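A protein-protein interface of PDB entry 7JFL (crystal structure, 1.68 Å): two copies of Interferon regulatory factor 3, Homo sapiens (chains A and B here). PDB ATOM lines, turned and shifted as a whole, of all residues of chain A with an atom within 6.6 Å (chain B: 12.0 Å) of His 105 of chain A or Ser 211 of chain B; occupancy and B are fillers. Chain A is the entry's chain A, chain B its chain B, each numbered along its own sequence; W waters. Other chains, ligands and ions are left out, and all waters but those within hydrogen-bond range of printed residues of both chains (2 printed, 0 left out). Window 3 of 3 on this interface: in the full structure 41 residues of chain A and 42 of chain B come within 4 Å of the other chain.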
ATOM      1  N   CYS A  82       4.082  22.255 -25.300  1.00  0.00           N
ATOM      2  CA  CYS A  82       5.193  21.382 -24.941  1.00  0.00           C
ATOM      3  C   CYS A  82       6.210  22.079 -24.050  1.00  0.00           C
ATOM      4  O   CYS A  82       7.300  21.535 -23.820  1.00  0.00           O
ATOM      5  CB  CYS A  82       5.874  20.847 -26.202  1.00  0.00           C
ATOM      6  SG  CYS A  82       4.786  19.850 -27.225  1.00  0.00           S
ATOM      7  N   ARG A 100      15.756  24.542 -19.345  1.00  0.00           N
ATOM      8  CA  ARG A 100      14.614  24.132 -20.139  1.00  0.00           C
ATOM      9  C   ARG A 100      13.929  22.992 -19.387  1.00  0.00           C
ATOM     10  O   ARG A 100      14.517  21.922 -19.209  1.00  0.00           O
ATOM     11  CB  ARG A 100      15.106  23.718 -21.522  1.00  0.00           C
ATOM     12  CG  ARG A 100      14.066  23.690 -22.596  1.00  0.00           C
ATOM     13  CD  ARG A 100      13.817  22.266 -22.984  1.00  0.00           C
ATOM     14  NE  ARG A 100      14.971  21.601 -23.595  1.00  0.00           N
ATOM     15  CZ  ARG A 100      14.990  20.300 -23.865  1.00  0.00           C
ATOM     16  NH1 ARG A 100      13.931  19.565 -23.566  1.00  0.00           N
ATOM     17  NH2 ARG A 100      16.048  19.729 -24.429  1.00  0.00           N
ATOM     18  N   GLY A 102      10.774  21.770 -20.127  1.00  0.00           N
ATOM     19  CA  GLY A 102       9.831  21.036 -20.946  1.00  0.00           C
ATOM     20  C   GLY A 102      10.500  20.404 -22.149  1.00  0.00           C
ATOM     21  O   GLY A 102      11.697  20.110 -22.110  1.00  0.00           O
ATOM     22  N   HIS A 103       9.748  20.191 -23.229  1.00  0.00           N
ATOM     23  CA  HIS A 103      10.235  19.385 -24.342  1.00  0.00           C
ATOM     24  C   HIS A 103      10.688  20.203 -25.544  1.00  0.00           C
ATOM     25  O   HIS A 103      11.287  19.633 -26.460  1.00  0.00           O
ATOM     26  CB  HIS A 103       9.150  18.399 -24.795  1.00  0.00           C
ATOM     27  CG  HIS A 103       8.743  17.422 -23.741  1.00  0.00           C
ATOM     28  ND1 HIS A 103       8.066  17.796 -22.600  1.00  0.00           N
ATOM     29  CD2 HIS A 103       8.902  16.079 -23.661  1.00  0.00           C
ATOM     30  CE1 HIS A 103       7.831  16.726 -21.859  1.00  0.00           C
ATOM     31  NE2 HIS A 103       8.326  15.671 -22.481  1.00  0.00           N
ATOM     32  N   CYS A 104      10.411  21.506 -25.575  1.00  0.00           N
ATOM     33  CA  CYS A 104      10.827  22.347 -26.696  1.00  0.00           C
ATOM     34  C   CYS A 104      12.305  22.681 -26.558  1.00  0.00           C
ATOM     35  O   CYS A 104      12.706  23.396 -25.633  1.00  0.00           O
ATOM     36  CB  CYS A 104      10.012  23.637 -26.758  1.00  0.00           C
ATOM     37  SG  CYS A 104       8.251  23.376 -26.890  1.00  0.00           S
ATOM     38  N   HIS A 105      13.119  22.200 -27.492  1.00  0.00           N
ATOM     39  CA  HIS A 105      14.487  22.692 -27.581  1.00  0.00           C
ATOM     40  C   HIS A 105      14.483  24.206 -27.778  1.00  0.00           C
ATOM     41  O   HIS A 105      13.710  24.736 -28.576  1.00  0.00           O
ATOM     42  CB  HIS A 105      15.216  22.011 -28.740  1.00  0.00           C
ATOM     43  CG  HIS A 105      15.458  20.554 -28.518  1.00  0.00           C
ATOM     44  ND1 HIS A 105      16.717  20.033 -28.305  1.00  0.00           N
ATOM     45  CD2 HIS A 105      14.602  19.511 -28.440  1.00  0.00           C
ATOM     46  CE1 HIS A 105      16.627  18.728 -28.127  1.00  0.00           C
ATOM     47  NE2 HIS A 105      15.353  18.386 -28.197  1.00  0.00           N
ATOM     48  N   THR A 106      15.347  24.909 -27.043  1.00  0.00           N
ATOM     49  CA  THR A 106      15.373  26.371 -27.096  1.00  0.00           C
ATOM     50  C   THR A 106      16.803  26.851 -27.282  1.00  0.00           C
ATOM     51  O   THR A 106      17.702  26.410 -26.561  1.00  0.00           O
ATOM     52  CB  THR A 106      14.772  26.979 -25.824  1.00  0.00           C
ATOM     53  OG1 THR A 106      13.393  26.594 -25.707  1.00  0.00           O
ATOM     54  CG2 THR A 106      14.883  28.502 -25.850  1.00  0.00           C
ATOM     55  N   TYR A 107      17.019  27.742 -28.250  1.00  0.00           N
ATOM     56  CA  TYR A 107      18.353  28.242 -28.551  1.00  0.00           C
ATOM     57  C   TYR A 107      18.390  29.737 -28.287  1.00  0.00           C
ATOM     58  O   TYR A 107      17.395  30.442 -28.481  1.00  0.00           O
ATOM     59  CB  TYR A 107      18.760  27.944 -29.996  1.00  0.00           C
ATOM     60  CG  TYR A 107      18.555  26.483 -30.336  1.00  0.00           C
ATOM     61  CD1 TYR A 107      17.320  26.031 -30.795  1.00  0.00           C
ATOM     62  CD2 TYR A 107      19.568  25.556 -30.144  1.00  0.00           C
ATOM     63  CE1 TYR A 107      17.107  24.694 -31.072  1.00  0.00           C
ATOM     64  CE2 TYR A 107      19.365  24.215 -30.435  1.00  0.00           C
ATOM     65  CZ  TYR A 107      18.125  23.799 -30.889  1.00  0.00           C
ATOM     66  OH  TYR A 107      17.891  22.474 -31.173  1.00  0.00           O
ATOM     67  N   GLU A 125      22.555  26.397 -26.705  1.00  0.00           N
ATOM     68  CA  GLU A 125      21.253  25.782 -26.479  1.00  0.00           C
ATOM     69  C   GLU A 125      20.988  25.714 -24.982  1.00  0.00           C
ATOM     70  O   GLU A 125      21.875  25.350 -24.202  1.00  0.00           O
ATOM     71  CB  GLU A 125      21.173  24.368 -27.063  1.00  0.00           C
ATOM     72  CG  GLU A 125      19.761  23.798 -26.962  1.00  0.00           C
ATOM     73  CD  GLU A 125      19.639  22.370 -27.468  1.00  0.00           C
ATOM     74  OE1 GLU A 125      20.599  21.851 -28.081  1.00  0.00           O
ATOM     75  OE2 GLU A 125      18.570  21.763 -27.255  1.00  0.00           O
ATOM     76  N   VAL A 126      19.762  26.052 -24.583  1.00  0.00           N
ATOM     77  CA  VAL A 126      19.386  25.989 -23.174  1.00  0.00           C
ATOM     78  C   VAL A 126      19.351  24.536 -22.715  1.00  0.00           C
ATOM     79  O   VAL A 126      18.627  23.709 -23.286  1.00  0.00           O
ATOM     80  CB  VAL A 126      18.029  26.663 -22.922  1.00  0.00           C
ATOM     81  CG1 VAL A 126      17.661  26.557 -21.442  1.00  0.00           C
ATOM     82  CG2 VAL A 126      18.049  28.134 -23.408  1.00  0.00           C
ATOM     83  N   CYS A 162      14.956  31.372 -29.173  1.00  0.00           N
ATOM     84  CA  CYS A 162      14.196  30.763 -30.259  1.00  0.00           C
ATOM     85  C   CYS A 162      13.653  29.444 -29.729  1.00  0.00           C
ATOM     86  O   CYS A 162      14.429  28.561 -29.357  1.00  0.00           O
ATOM     87  CB  CYS A 162      15.071  30.546 -31.494  1.00  0.00           C
ATOM     88  SG  CYS A 162      14.137  29.946 -32.913  1.00  0.00           S
ATOM     89  N   VAL A 163      12.329  29.322 -29.656  1.00  0.00           N
ATOM     90  CA  VAL A 163      11.678  28.230 -28.926  1.00  0.00           C
ATOM     91  C   VAL A 163      11.070  27.252 -29.924  1.00  0.00           C
ATOM     92  O   VAL A 163      10.194  27.623 -30.717  1.00  0.00           O
ATOM     93  CB  VAL A 163      10.604  28.755 -27.954  1.00  0.00           C
ATOM     94  CG1 VAL A 163       9.966  27.604 -27.214  1.00  0.00           C
ATOM     95  CG2 VAL A 163      11.204  29.753 -26.965  1.00  0.00           C
ATOM     96  N   GLY A 164      11.531  26.003 -29.877  1.00  0.00           N
ATOM     97  CA  GLY A 164      10.932  24.917 -30.630  1.00  0.00           C
ATOM     98  C   GLY A 164      11.411  24.763 -32.059  1.00  0.00           C
ATOM     99  O   GLY A 164      10.900  23.884 -32.768  1.00  0.00           O
ATOM    100  N   GLU A 165      12.349  25.598 -32.505  1.00  0.00           N
ATOM    101  CA  GLU A 165      12.901  25.567 -33.852  1.00  0.00           C
ATOM    102  C   GLU A 165      14.381  25.903 -33.770  1.00  0.00           C
ATOM    103  O   GLU A 165      14.831  26.537 -32.816  1.00  0.00           O
ATOM    104  CB  GLU A 165      12.205  26.573 -34.767  1.00  0.00           C
ATOM    105  CG  GLU A 165      10.832  26.174 -35.244  1.00  0.00           C
ATOM    106  CD  GLU A 165      10.269  27.247 -36.120  1.00  0.00           C
ATOM    107  OE1 GLU A 165      10.368  27.098 -37.350  1.00  0.00           O
ATOM    108  OE2 GLU A 165       9.788  28.260 -35.568  1.00  0.00           O
ATOM    109  N   SER A 166      15.140  25.494 -34.781  1.00  0.00           N
ATOM    110  CA  SER A 166      16.545  25.877 -34.769  1.00  0.00           C
ATOM    111  C   SER A 166      16.683  27.391 -34.890  1.00  0.00           C
ATOM    112  O   SER A 166      15.767  28.095 -35.320  1.00  0.00           O
ATOM    113  CB  SER A 166      17.311  25.191 -35.896  1.00  0.00           C
ATOM    114  OG  SER A 166      16.786  25.564 -37.156  1.00  0.00           O
ATOM    115  N   VAL B 206       8.762  23.474 -42.309  1.00  0.00           N
ATOM    116  CA  VAL B 206       8.956  23.818 -40.909  1.00  0.00           C
ATOM    117  C   VAL B 206       9.252  22.543 -40.132  1.00  0.00           C
ATOM    118  O   VAL B 206       8.623  21.501 -40.352  1.00  0.00           O
ATOM    119  CB  VAL B 206       7.725  24.562 -40.363  1.00  0.00           C
ATOM    120  CG1 VAL B 206       6.472  23.724 -40.544  1.00  0.00           C
ATOM    121  CG2 VAL B 206       7.914  24.911 -38.894  1.00  0.00           C
ATOM    122  N   ASP B 207      10.252  22.605 -39.259  1.00  0.00           N
ATOM    123  CA  ASP B 207      10.750  21.425 -38.553  1.00  0.00           C
ATOM    124  C   ASP B 207      10.854  21.777 -37.075  1.00  0.00           C
ATOM    125  O   ASP B 207      11.799  22.451 -36.653  1.00  0.00           O
ATOM    126  CB  ASP B 207      12.093  20.972 -39.120  1.00  0.00           C
ATOM    127  CG  ASP B 207      12.572  19.660 -38.525  1.00  0.00           C
ATOM    128  OD1 ASP B 207      11.832  19.046 -37.723  1.00  0.00           O
ATOM    129  OD2 ASP B 207      13.693  19.232 -38.872  1.00  0.00           O
ATOM    130  N   LEU B 208       9.870  21.333 -36.296  1.00  0.00           N
ATOM    131  CA  LEU B 208       9.891  21.574 -34.861  1.00  0.00           C
ATOM    132  C   LEU B 208      10.960  20.719 -34.195  1.00  0.00           C
ATOM    133  O   LEU B 208      11.165  19.556 -34.554  1.00  0.00           O
ATOM    134  CB  LEU B 208       8.522  21.269 -34.248  1.00  0.00           C
ATOM    135  CG  LEU B 208       7.349  22.114 -34.754  1.00  0.00           C
ATOM    136  CD1 LEU B 208       6.054  21.765 -34.031  1.00  0.00           C
ATOM    137  CD2 LEU B 208       7.677  23.591 -34.598  1.00  0.00           C
ATOM    138  N   HIS B 209      11.646  21.299 -33.219  1.00  0.00           N
ATOM    139  CA  HIS B 209      12.628  20.588 -32.398  1.00  0.00           C
ATOM    140  C   HIS B 209      11.986  20.354 -31.033  1.00  0.00           C
ATOM    141  O   HIS B 209      12.187  21.143 -30.109  1.00  0.00           O
ATOM    142  CB  HIS B 209      13.928  21.392 -32.227  1.00  0.00           C
ATOM    143  CG  HIS B 209      14.728  21.578 -33.482  1.00  0.00           C
ATOM    144  ND1 HIS B 209      14.248  21.288 -34.739  1.00  0.00           N
ATOM    145  CD2 HIS B 209      15.999  22.018 -33.656  1.00  0.00           C
ATOM    146  CE1 HIS B 209      15.182  21.550 -35.636  1.00  0.00           C
ATOM    147  NE2 HIS B 209      16.257  21.990 -35.005  1.00  0.00           N
ATOM    148  N   ILE B 210      11.224  19.268 -30.898  1.00  0.00           N
ATOM    149  CA  ILE B 210      10.531  18.956 -29.651  1.00  0.00           C
ATOM    150  C   ILE B 210      10.794  17.500 -29.295  1.00  0.00           C
ATOM    151  O   ILE B 210      10.530  16.604 -30.103  1.00  0.00           O
ATOM    152  CB  ILE B 210       9.016  19.214 -29.751  1.00  0.00           C
ATOM    153  CG1 ILE B 210       8.734  20.685 -30.056  1.00  0.00           C
ATOM    154  CG2 ILE B 210       8.326  18.787 -28.461  1.00  0.00           C
ATOM    155  CD1 ILE B 210       7.268  20.988 -30.246  1.00  0.00           C
ATOM    156  N   SER B 211      11.281  17.267 -28.084  1.00  0.00           N
ATOM    157  CA  SER B 211      11.664  15.934 -27.626  1.00  0.00           C
ATOM    158  C   SER B 211      10.600  15.301 -26.731  1.00  0.00           C
ATOM    159  O   SER B 211       9.463  15.768 -26.674  1.00  0.00           O
ATOM    160  CB  SER B 211      12.991  16.003 -26.877  1.00  0.00           C
ATOM    161  OG  SER B 211      13.327  14.747 -26.309  1.00  0.00           O
HETATM  162  O   HOH W   1      13.763  24.245 -37.075  1.00  0.00           O
HETATM  163  O   HOH W   2      11.739  25.330 -38.796  1.00  0.00           O
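O of Gly 164 of chain A sits at hydrogen-bond distance from N of His 209 of chain B, at 2.7 Å. O of His 209 of chain B lies within hydrogen-bond range of N of His 105 of chain A (3.0 Å). O of His 103 of chain A lies within hydrogen-bond range of N of Ser 211 of chain B (2.9 Å).
The backbone carbonyl oxygen (O) of His 105 of chain A is in hydrogen-bond range of the backbone NH (N) of Gly 164 of chain A (2.8 Å). ND1 of His 105 of chain A lies within hydrogen-bond range of OE2 of Glu 125 of chain A (2.7 Å). OG1 of Thr 106 of chain A is in hydrogen-bond range of O of Cys 104 of chain A, at 3.3 Å. SG of Cys 104 of chain A sits close to O of Cys 82 of chain A, at 3.7 Å. The side-chain sulfur of Cys 162 of chain A is in hydrogen-bond range of the backbone carbonyl oxygen of Ser 166 of chain A, at 3.4 Å. O of Tyr 107 of chain A sits at hydrogen-bond distance from N of Cys 162 of chain A.
Among the printed residues, merely in contact across the chains: Tyr 107 of chain A with His 209 of chain B, Gly 164 of chain A with Leu 208 of chain B, His 103 of chain A with Ile 210 of chain B, Ser 166 of chain A with His 209 of chain B, His 105 of chain A with Ser 211 of chain B, Glu 165 of chain A with Val 206 of chain B, Cys 104 of chain A with His 209 of chain B and Cys 82 of chain A with Ile 210 of chain B.
Of the printed residues of chain B, Cys 82 of chain A touches Ile 210 (3.9 Å). No residue of chain B comes within 4 Å of Gly 102 of chain A. His 103 of chain A touches just these residues of chain B: Ile 210 and Ser 211. His 105 of chain A touches just these residues of chain B: His 209 (3.0 Å) and Ser 211 (3.6 Å). Glu 125 of chain A touches none of the printed residues of chain B. No residue of chain B comes within 4 Å of Val 126 of chain A. No residue of chain B comes within 4 Å of Val 163 of chain A. Gly 164 of chain A touches two residues of chain B. Of the printed residues of chain B, Glu 165 of chain A touches Val 206. Printed residues of chain A within 4 Å of Ser 211 of chain B: His 103 (2.9 Å) and His 105 (3.6 Å). The nearest residue of chain B that does not touch His 105 of chain A is Ile 210 of chain B (4.2 Å). The nearest printed residue of chain A that does not touch Ile 210 of chain B is Cys 104 of chain A (4.2 Å).
Of the 6 printed residues of chain B, 5 touch a printed residue of chain A. Hydrophobic or aromatic side chains of chain B that line the printed part of chain A: Val 206, Leu 208, His 209 and Ile 210. Hydrophobic or aromatic side chains of chain A that line the printed part of chain B: His 103, His 105 and Tyr 107. Among the printed residues, no Asp or Glu carboxylate lies within 4 Å of a Lys or Arg side-chain nitrogen of the other chain.
No position is printed for both chains. Of the 11 pairs that touch across the chains among the printed residues, none has its exchanged pair printed and touching as well.
Water W2 bridges the side-chain carboxylate of Glu 165 of chain A and the backbone NH of Asp 207 of chain B. Water W1 lies within hydrogen-bond range of the backbone carbonyl oxygen (O) of Asp 207 of chain B (2.7 Å) and the backbone NH (N) of Ser 166 of chain A (3.0 Å).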
